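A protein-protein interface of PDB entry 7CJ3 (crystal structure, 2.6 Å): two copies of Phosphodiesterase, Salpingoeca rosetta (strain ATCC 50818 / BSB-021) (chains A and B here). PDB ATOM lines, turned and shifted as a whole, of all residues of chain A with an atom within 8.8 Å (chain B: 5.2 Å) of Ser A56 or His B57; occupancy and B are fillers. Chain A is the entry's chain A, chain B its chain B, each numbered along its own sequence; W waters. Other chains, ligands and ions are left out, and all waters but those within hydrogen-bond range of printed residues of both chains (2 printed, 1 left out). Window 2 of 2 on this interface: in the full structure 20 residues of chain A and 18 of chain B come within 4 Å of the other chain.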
ATOM      1  N   ARG A  49      -6.167  19.763   2.041  1.00  0.00           N
ATOM      2  CA  ARG A  49      -5.568  20.150   0.734  1.00  0.00           C
ATOM      3  C   ARG A  49      -5.557  18.915  -0.188  1.00  0.00           C
ATOM      4  O   ARG A  49      -5.940  19.062  -1.364  1.00  0.00           O
ATOM      5  CB  ARG A  49      -4.185  20.768   0.971  1.00  0.00           C
ATOM      6  N   ARG A  50      -5.171  17.746   0.326  1.00  0.00           N
ATOM      7  CA  ARG A  50      -5.080  16.469  -0.437  1.00  0.00           C
ATOM      8  C   ARG A  50      -6.484  15.949  -0.800  1.00  0.00           C
ATOM      9  O   ARG A  50      -6.647  15.378  -1.910  1.00  0.00           O
ATOM     10  CB  ARG A  50      -4.353  15.391   0.386  1.00  0.00           C
ATOM     11  CG  ARG A  50      -2.865  15.620   0.603  1.00  0.00           C
ATOM     12  CD  ARG A  50      -2.077  16.018  -0.644  1.00  0.00           C
ATOM     13  NE  ARG A  50      -1.321  14.951  -1.296  1.00  0.00           N
ATOM     14  CZ  ARG A  50      -0.048  14.655  -1.039  1.00  0.00           C
ATOM     15  NH1 ARG A  50       0.623  15.316  -0.107  1.00  0.00           N
ATOM     16  NH2 ARG A  50       0.552  13.690  -1.715  1.00  0.00           N
ATOM     17  N   VAL A  51      -7.460  16.131   0.094  1.00  0.00           N
ATOM     18  CA  VAL A  51      -8.869  15.695  -0.116  1.00  0.00           C
ATOM     19  C   VAL A  51      -9.442  16.486  -1.288  1.00  0.00           C
ATOM     20  O   VAL A  51     -10.017  15.848  -2.209  1.00  0.00           O
ATOM     21  CB  VAL A  51      -9.734  15.836   1.144  1.00  0.00           C
ATOM     22  CG1 VAL A  51     -11.215  15.883   0.819  1.00  0.00           C
ATOM     23  CG2 VAL A  51      -9.444  14.728   2.129  1.00  0.00           C
ATOM     24  N   PHE A  52      -9.287  17.811  -1.248  1.00  0.00           N
ATOM     25  CA  PHE A  52      -9.838  18.748  -2.259  1.00  0.00           C
ATOM     26  C   PHE A  52      -9.015  18.653  -3.553  1.00  0.00           C
ATOM     27  O   PHE A  52      -9.554  19.014  -4.591  1.00  0.00           O
ATOM     28  CB  PHE A  52      -9.956  20.160  -1.687  1.00  0.00           C
ATOM     29  CG  PHE A  52     -11.055  20.344  -0.670  1.00  0.00           C
ATOM     30  CD1 PHE A  52     -12.383  20.117  -1.018  1.00  0.00           C
ATOM     31  CD2 PHE A  52     -10.784  20.749   0.634  1.00  0.00           C
ATOM     32  CE1 PHE A  52     -13.408  20.322  -0.096  1.00  0.00           C
ATOM     33  CE2 PHE A  52     -11.806  20.924   1.556  1.00  0.00           C
ATOM     34  CZ  PHE A  52     -13.115  20.733   1.185  1.00  0.00           C
ATOM     35  N   ALA A  53      -7.781  18.145  -3.505  1.00  0.00           N
ATOM     36  CA  ALA A  53      -6.933  17.892  -4.694  1.00  0.00           C
ATOM     37  C   ALA A  53      -7.323  16.559  -5.361  1.00  0.00           C
ATOM     38  O   ALA A  53      -7.261  16.480  -6.598  1.00  0.00           O
ATOM     39  CB  ALA A  53      -5.477  17.908  -4.318  1.00  0.00           C
ATOM     40  N   LYS A  54      -7.698  15.539  -4.590  1.00  0.00           N
ATOM     41  CA  LYS A  54      -8.116  14.222  -5.137  1.00  0.00           C
ATOM     42  C   LYS A  54      -9.537  14.348  -5.713  1.00  0.00           C
ATOM     43  O   LYS A  54      -9.898  13.560  -6.622  1.00  0.00           O
ATOM     44  CB  LYS A  54      -8.030  13.161  -4.030  1.00  0.00           C
ATOM     45  CG  LYS A  54      -8.322  11.723  -4.442  1.00  0.00           C
ATOM     46  CD  LYS A  54      -8.630  10.826  -3.226  1.00  0.00           C
ATOM     47  CE  LYS A  54      -8.620   9.346  -3.494  1.00  0.00           C
ATOM     48  NZ  LYS A  54      -7.213   8.892  -3.501  1.00  0.00           N
ATOM     49  N   PHE A  55     -10.317  15.292  -5.180  1.00  0.00           N
ATOM     50  CA  PHE A  55     -11.770  15.462  -5.437  1.00  0.00           C
ATOM     51  C   PHE A  55     -12.025  16.938  -5.752  1.00  0.00           C
ATOM     52  O   PHE A  55     -12.355  17.714  -4.814  1.00  0.00           O
ATOM     53  CB  PHE A  55     -12.571  15.031  -4.206  1.00  0.00           C
ATOM     54  CG  PHE A  55     -12.418  13.593  -3.764  1.00  0.00           C
ATOM     55  CD1 PHE A  55     -12.486  12.543  -4.673  1.00  0.00           C
ATOM     56  CD2 PHE A  55     -12.264  13.275  -2.419  1.00  0.00           C
ATOM     57  CE1 PHE A  55     -12.365  11.226  -4.253  1.00  0.00           C
ATOM     58  CE2 PHE A  55     -12.175  11.959  -1.998  1.00  0.00           C
ATOM     59  CZ  PHE A  55     -12.220  10.938  -2.920  1.00  0.00           C
ATOM     60  N   SER A  56     -11.854  17.326  -7.018  1.00  0.00           N
ATOM     61  CA  SER A  56     -11.738  18.749  -7.433  1.00  0.00           C
ATOM     62  C   SER A  56     -13.105  19.424  -7.564  1.00  0.00           C
ATOM     63  O   SER A  56     -13.115  20.644  -7.692  1.00  0.00           O
ATOM     64  CB  SER A  56     -10.887  18.900  -8.646  1.00  0.00           C
ATOM     65  OG  SER A  56     -11.188  17.926  -9.597  1.00  0.00           O
ATOM     66  N   HIS A  57     -14.212  18.699  -7.495  1.00  0.00           N
ATOM     67  CA  HIS A  57     -15.569  19.272  -7.701  1.00  0.00           C
ATOM     68  C   HIS A  57     -16.202  19.669  -6.364  1.00  0.00           C
ATOM     69  O   HIS A  57     -17.230  20.386  -6.390  1.00  0.00           O
ATOM     70  CB  HIS A  57     -16.431  18.321  -8.544  1.00  0.00           C
ATOM     71  CG  HIS A  57     -15.738  17.889  -9.794  1.00  0.00           C
ATOM     72  ND1 HIS A  57     -15.730  18.688 -10.956  1.00  0.00           N
ATOM     73  CD2 HIS A  57     -15.042  16.774 -10.110  1.00  0.00           C
ATOM     74  CE1 HIS A  57     -15.051  18.076 -11.904  1.00  0.00           C
ATOM     75  NE2 HIS A  57     -14.637  16.906 -11.417  1.00  0.00           N
ATOM     76  N   LEU A  58     -15.574  19.275  -5.243  1.00  0.00           N
ATOM     77  CA  LEU A  58     -16.194  19.343  -3.891  1.00  0.00           C
ATOM     78  C   LEU A  58     -16.394  20.816  -3.468  1.00  0.00           C
ATOM     79  O   LEU A  58     -17.503  21.109  -2.962  1.00  0.00           O
ATOM     80  CB  LEU A  58     -15.344  18.532  -2.912  1.00  0.00           C
ATOM     81  CG  LEU A  58     -15.450  17.021  -3.062  1.00  0.00           C
ATOM     82  CD1 LEU A  58     -14.745  16.281  -1.928  1.00  0.00           C
ATOM     83  CD2 LEU A  58     -16.889  16.589  -3.109  1.00  0.00           C
ATOM     84  N   GLN A  59     -15.432  21.716  -3.729  1.00  0.00           N
ATOM     85  CA  GLN A  59     -15.548  23.141  -3.332  1.00  0.00           C
ATOM     86  C   GLN A  59     -16.752  23.761  -4.082  1.00  0.00           C
ATOM     87  O   GLN A  59     -17.594  24.470  -3.481  1.00  0.00           O
ATOM     88  CB  GLN A  59     -14.207  23.851  -3.528  1.00  0.00           C
ATOM     89  CG  GLN A  59     -13.151  23.434  -2.489  1.00  0.00           C
ATOM     90  CD  GLN A  59     -12.038  24.422  -2.145  1.00  0.00           C
ATOM     91  OE1 GLN A  59     -11.494  24.431  -1.021  1.00  0.00           O
ATOM     92  NE2 GLN A  59     -11.630  25.243  -3.111  1.00  0.00           N
ATOM     93  N   SER A  60     -16.873  23.441  -5.363  1.00  0.00           N
ATOM     94  CA  SER A  60     -17.957  23.959  -6.234  1.00  0.00           C
ATOM     95  C   SER A  60     -19.302  23.535  -5.678  1.00  0.00           C
ATOM     96  O   SER A  60     -20.194  24.378  -5.622  1.00  0.00           O
ATOM     97  CB  SER A  60     -17.769  23.533  -7.641  1.00  0.00           C
ATOM     98  OG  SER A  60     -16.418  23.800  -8.015  1.00  0.00           O
ATOM     99  N   PHE A  61     -19.422  22.255  -5.308  1.00  0.00           N
ATOM    100  CA  PHE A  61     -20.671  21.653  -4.789  1.00  0.00           C
ATOM    101  C   PHE A  61     -21.124  22.400  -3.534  1.00  0.00           C
ATOM    102  O   PHE A  61     -22.255  22.909  -3.505  1.00  0.00           O
ATOM    103  CB  PHE A  61     -20.458  20.166  -4.515  1.00  0.00           C
ATOM    104  CG  PHE A  61     -20.198  19.300  -5.723  1.00  0.00           C
ATOM    105  CD1 PHE A  61     -20.294  19.804  -7.026  1.00  0.00           C
ATOM    106  CD2 PHE A  61     -19.914  17.951  -5.558  1.00  0.00           C
ATOM    107  CE1 PHE A  61     -20.035  18.996  -8.116  1.00  0.00           C
ATOM    108  CE2 PHE A  61     -19.684  17.142  -6.657  1.00  0.00           C
ATOM    109  CZ  PHE A  61     -19.739  17.668  -7.935  1.00  0.00           C
ATOM    110  N   ALA A  64     -21.848  26.166  -4.207  1.00  0.00           N
ATOM    111  CA  ALA A  64     -23.132  26.292  -4.935  1.00  0.00           C
ATOM    112  C   ALA A  64     -24.288  26.064  -3.964  1.00  0.00           C
ATOM    113  O   ALA A  64     -25.266  26.829  -4.003  1.00  0.00           O
ATOM    114  CB  ALA A  64     -23.185  25.295  -6.055  1.00  0.00           C
ATOM    115  N   PHE A 250     -17.173   8.839  -4.553  1.00  0.00           N
ATOM    116  CA  PHE A 250     -17.385   9.789  -3.441  1.00  0.00           C
ATOM    117  C   PHE A 250     -18.113  11.034  -3.932  1.00  0.00           C
ATOM    118  O   PHE A 250     -19.190  11.391  -3.342  1.00  0.00           O
ATOM    119  CB  PHE A 250     -16.041  10.165  -2.817  1.00  0.00           C
ATOM    120  CG  PHE A 250     -16.234  10.960  -1.565  1.00  0.00           C
ATOM    121  CD1 PHE A 250     -16.901  10.392  -0.486  1.00  0.00           C
ATOM    122  CD2 PHE A 250     -15.840  12.293  -1.494  1.00  0.00           C
ATOM    123  CE1 PHE A 250     -17.129  11.143   0.660  1.00  0.00           C
ATOM    124  CE2 PHE A 250     -16.061  13.028  -0.343  1.00  0.00           C
ATOM    125  CZ  PHE A 250     -16.707  12.455   0.729  1.00  0.00           C
ATOM    126  N   GLN A 251     -17.544  11.651  -4.982  1.00  0.00           N
ATOM    127  CA  GLN A 251     -18.009  12.918  -5.612  1.00  0.00           C
ATOM    128  C   GLN A 251     -19.452  12.773  -6.116  1.00  0.00           C
ATOM    129  O   GLN A 251     -20.249  13.696  -5.867  1.00  0.00           O
ATOM    130  CB  GLN A 251     -17.049  13.352  -6.715  1.00  0.00           C
ATOM    131  CG  GLN A 251     -15.650  13.696  -6.179  1.00  0.00           C
ATOM    132  CD  GLN A 251     -14.823  14.559  -7.097  1.00  0.00           C
ATOM    133  OE1 GLN A 251     -14.137  14.073  -7.984  1.00  0.00           O
ATOM    134  NE2 GLN A 251     -14.864  15.853  -6.865  1.00  0.00           N
ATOM    135  N   PHE B  55     -11.150  23.164 -17.999  1.00  0.00           N
ATOM    136  CA  PHE B  55     -12.005  23.933 -17.059  1.00  0.00           C
ATOM    137  C   PHE B  55     -12.950  22.947 -16.374  1.00  0.00           C
ATOM    138  O   PHE B  55     -14.086  22.751 -16.857  1.00  0.00           O
ATOM    139  CB  PHE B  55     -12.798  24.992 -17.823  1.00  0.00           C
ATOM    140  CG  PHE B  55     -11.997  26.040 -18.568  1.00  0.00           C
ATOM    141  CD1 PHE B  55     -10.930  26.694 -17.967  1.00  0.00           C
ATOM    142  CD2 PHE B  55     -12.354  26.420 -19.856  1.00  0.00           C
ATOM    143  CE1 PHE B  55     -10.232  27.684 -18.638  1.00  0.00           C
ATOM    144  CE2 PHE B  55     -11.654  27.415 -20.526  1.00  0.00           C
ATOM    145  CZ  PHE B  55     -10.595  28.047 -19.916  1.00  0.00           C
ATOM    146  N   SER B  56     -12.483  22.317 -15.289  1.00  0.00           N
ATOM    147  CA  SER B  56     -13.100  21.112 -14.686  1.00  0.00           C
ATOM    148  C   SER B  56     -14.304  21.458 -13.811  1.00  0.00           C
ATOM    149  O   SER B  56     -15.027  20.532 -13.444  1.00  0.00           O
ATOM    150  CB  SER B  56     -12.078  20.416 -13.860  1.00  0.00           C
ATOM    151  OG  SER B  56     -10.884  21.120 -13.995  1.00  0.00           O
ATOM    152  N   HIS B  57     -14.538  22.723 -13.487  1.00  0.00           N
ATOM    153  CA  HIS B  57     -15.620  23.135 -12.556  1.00  0.00           C
ATOM    154  C   HIS B  57     -16.894  23.489 -13.322  1.00  0.00           C
ATOM    155  O   HIS B  57     -17.952  23.613 -12.666  1.00  0.00           O
ATOM    156  CB  HIS B  57     -15.117  24.237 -11.611  1.00  0.00           C
ATOM    157  CG  HIS B  57     -13.818  23.887 -10.964  1.00  0.00           C
ATOM    158  ND1 HIS B  57     -13.651  22.752 -10.166  1.00  0.00           N
ATOM    159  CD2 HIS B  57     -12.593  24.433 -11.119  1.00  0.00           C
ATOM    160  CE1 HIS B  57     -12.384  22.646  -9.810  1.00  0.00           C
ATOM    161  NE2 HIS B  57     -11.717  23.683 -10.353  1.00  0.00           N
ATOM    162  N   LEU B  58     -16.809  23.578 -14.655  1.00  0.00           N
ATOM    163  CA  LEU B  58     -17.877  24.160 -15.516  1.00  0.00           C
ATOM    164  C   LEU B  58     -19.142  23.289 -15.474  1.00  0.00           C
ATOM    165  O   LEU B  58     -20.236  23.869 -15.322  1.00  0.00           O
ATOM    166  CB  LEU B  58     -17.326  24.397 -16.924  1.00  0.00           C
ATOM    167  CG  LEU B  58     -16.350  25.571 -17.037  1.00  0.00           C
ATOM    168  CD1 LEU B  58     -15.996  25.885 -18.485  1.00  0.00           C
ATOM    169  CD2 LEU B  58     -16.933  26.804 -16.406  1.00  0.00           C
ATOM    170  N   GLN B  59     -19.024  21.962 -15.530  1.00  0.00           N
ATOM    171  CA  GLN B  59     -20.199  21.036 -15.520  1.00  0.00           C
ATOM    172  C   GLN B  59     -20.928  21.209 -14.178  1.00  0.00           C
ATOM    173  O   GLN B  59     -22.173  21.331 -14.149  1.00  0.00           O
ATOM    174  CB  GLN B  59     -19.694  19.610 -15.825  1.00  0.00           C
ATOM    175  CG  GLN B  59     -20.732  18.500 -15.880  1.00  0.00           C
ATOM    176  CD  GLN B  59     -20.043  17.175 -16.146  1.00  0.00           C
ATOM    177  OE1 GLN B  59     -18.826  17.132 -16.402  1.00  0.00           O
ATOM    178  NE2 GLN B  59     -20.827  16.103 -16.097  1.00  0.00           N
ATOM    179  N   SER B  60     -20.180  21.297 -13.087  1.00  0.00           N
ATOM    180  CA  SER B  60     -20.731  21.454 -11.721  1.00  0.00           C
ATOM    181  C   SER B  60     -21.542  22.729 -11.648  1.00  0.00           C
ATOM    182  O   SER B  60     -22.640  22.687 -11.101  1.00  0.00           O
ATOM    183  CB  SER B  60     -19.619  21.507 -10.717  1.00  0.00           C
ATOM    184  OG  SER B  60     -18.985  20.240 -10.583  1.00  0.00           O
ATOM    185  N   PHE B  61     -20.981  23.828 -12.167  1.00  0.00           N
ATOM    186  CA  PHE B  61     -21.602  25.174 -12.140  1.00  0.00           C
ATOM    187  C   PHE B  61     -22.956  25.132 -12.854  1.00  0.00           C
ATOM    188  O   PHE B  61     -23.973  25.486 -12.240  1.00  0.00           O
ATOM    189  CB  PHE B  61     -20.656  26.188 -12.770  1.00  0.00           C
ATOM    190  CG  PHE B  61     -19.366  26.450 -12.036  1.00  0.00           C
ATOM    191  CD1 PHE B  61     -19.112  25.906 -10.786  1.00  0.00           C
ATOM    192  CD2 PHE B  61     -18.418  27.298 -12.590  1.00  0.00           C
ATOM    193  CE1 PHE B  61     -17.905  26.148 -10.136  1.00  0.00           C
ATOM    194  CE2 PHE B  61     -17.220  27.552 -11.938  1.00  0.00           C
ATOM    195  CZ  PHE B  61     -16.968  26.974 -10.712  1.00  0.00           C
ATOM    196  N   GLN B 251     -13.266  30.569 -15.555  1.00  0.00           N
ATOM    197  CA  GLN B 251     -14.046  29.814 -14.534  1.00  0.00           C
ATOM    198  C   GLN B 251     -14.586  30.758 -13.444  1.00  0.00           C
ATOM    199  O   GLN B 251     -15.768  30.623 -13.088  1.00  0.00           O
ATOM    200  CB  GLN B 251     -13.205  28.679 -13.945  1.00  0.00           C
ATOM    201  CG  GLN B 251     -12.837  27.618 -14.954  1.00  0.00           C
ATOM    202  CD  GLN B 251     -12.461  26.274 -14.376  1.00  0.00           C
ATOM    203  OE1 GLN B 251     -11.318  26.026 -14.031  1.00  0.00           O
ATOM    204  NE2 GLN B 251     -13.418  25.377 -14.289  1.00  0.00           N
HETATM  205  O   HOH W   1     -15.763  21.433 -10.346  1.00  0.00           O
HETATM  206  O   HOH W   2     -17.065  16.935 -13.839  1.00  0.00           O
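ND1 of His B57 sits close to O of Ser A56, 3.3 Å away.
ND1 of His A57 lies close to O of Ser B56, at 3.2 Å.
Ser A56 touches His B57, and with the chains exchanged His A57 touches Ser B56.
His A57 touches Ser B60, and with the chains exchanged Ser A60 touches His B57.
Ser A60 touches Phe B61, and with the chains exchanged Phe A61 touches Ser B60.
Positions printed for both chains: 55, 56, 57, 58, 59, 60, 61 and 251.
Of the 6 pairs that touch across the chains among the printed residues, 6 have their exchanged pair printed and touching as well.
Among the printed residues, merely in contact across the chains: His A57 with Ser B60, Ser A60 with His B57, Ser A60 with Phe B61 and Phe A61 with Ser B60.
Along chain A the printed residues that touch a printed residue of chain B span positions 56 to 61.
Printed residues of chain B that touch a printed residue of chain A: Ser B56, His B57, Ser B60 and Phe B61.
Among the printed residues, no Asp or Glu carboxylate lies within 4 Å of a Lys or Arg side-chain nitrogen of the other chain.
The side-chain amide nitrogen of Gln A251 lies close to the backbone NH of Ser A56 (3.4 Å).
The backbone NH (N) of His A57 lies close to the side-chain amide nitrogen (NE2) of Gln A251, 3.0 Å away.
The side-chain amide nitrogen of Gln B251 sits close to the backbone NH of Ser B56 (3.4 Å).
The backbone NH (N) of His B57 sits close to the side-chain amide nitrogen (NE2) of Gln B251.
Water W1 lies within hydrogen-bond range of a ring nitrogen (ND1) of His B57 (2.5 Å), a ring nitrogen (ND1) of His A57 (2.8 Å), the backbone carbonyl oxygen of Ser B56 (3.3 Å), the side-chain hydroxyl of Ser A60 (3.4 Å) and the side-chain hydroxyl of Ser B60 (3.4 Å).
Water W2 bridges OE1 of Gln B59 and NE2 of His A57.
Ser A56 touches just one residue of chain B: His B57 (3.0 Å).
Printed residues of chain B within 4 Å of His A57: Ser B56 (2.9 Å) and Ser B60 (3.6 Å).
Gln A59 touches none of the printed residues of chain B.
Of the printed residues of chain A, Ser B56 touches His A57.
Of the printed residues of chain A, Ser B60 touches His A57 (3.6 Å) and Phe A61 (3.0 Å).
Gln B251 touches none of the printed residues of chain A.
The nearest residue of chain A that does not touch His B57 is His A57 (4.6 Å).
The nearest printed residue of chain A that does not touch Ser B60 is Ser A60 (4.1 Å).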
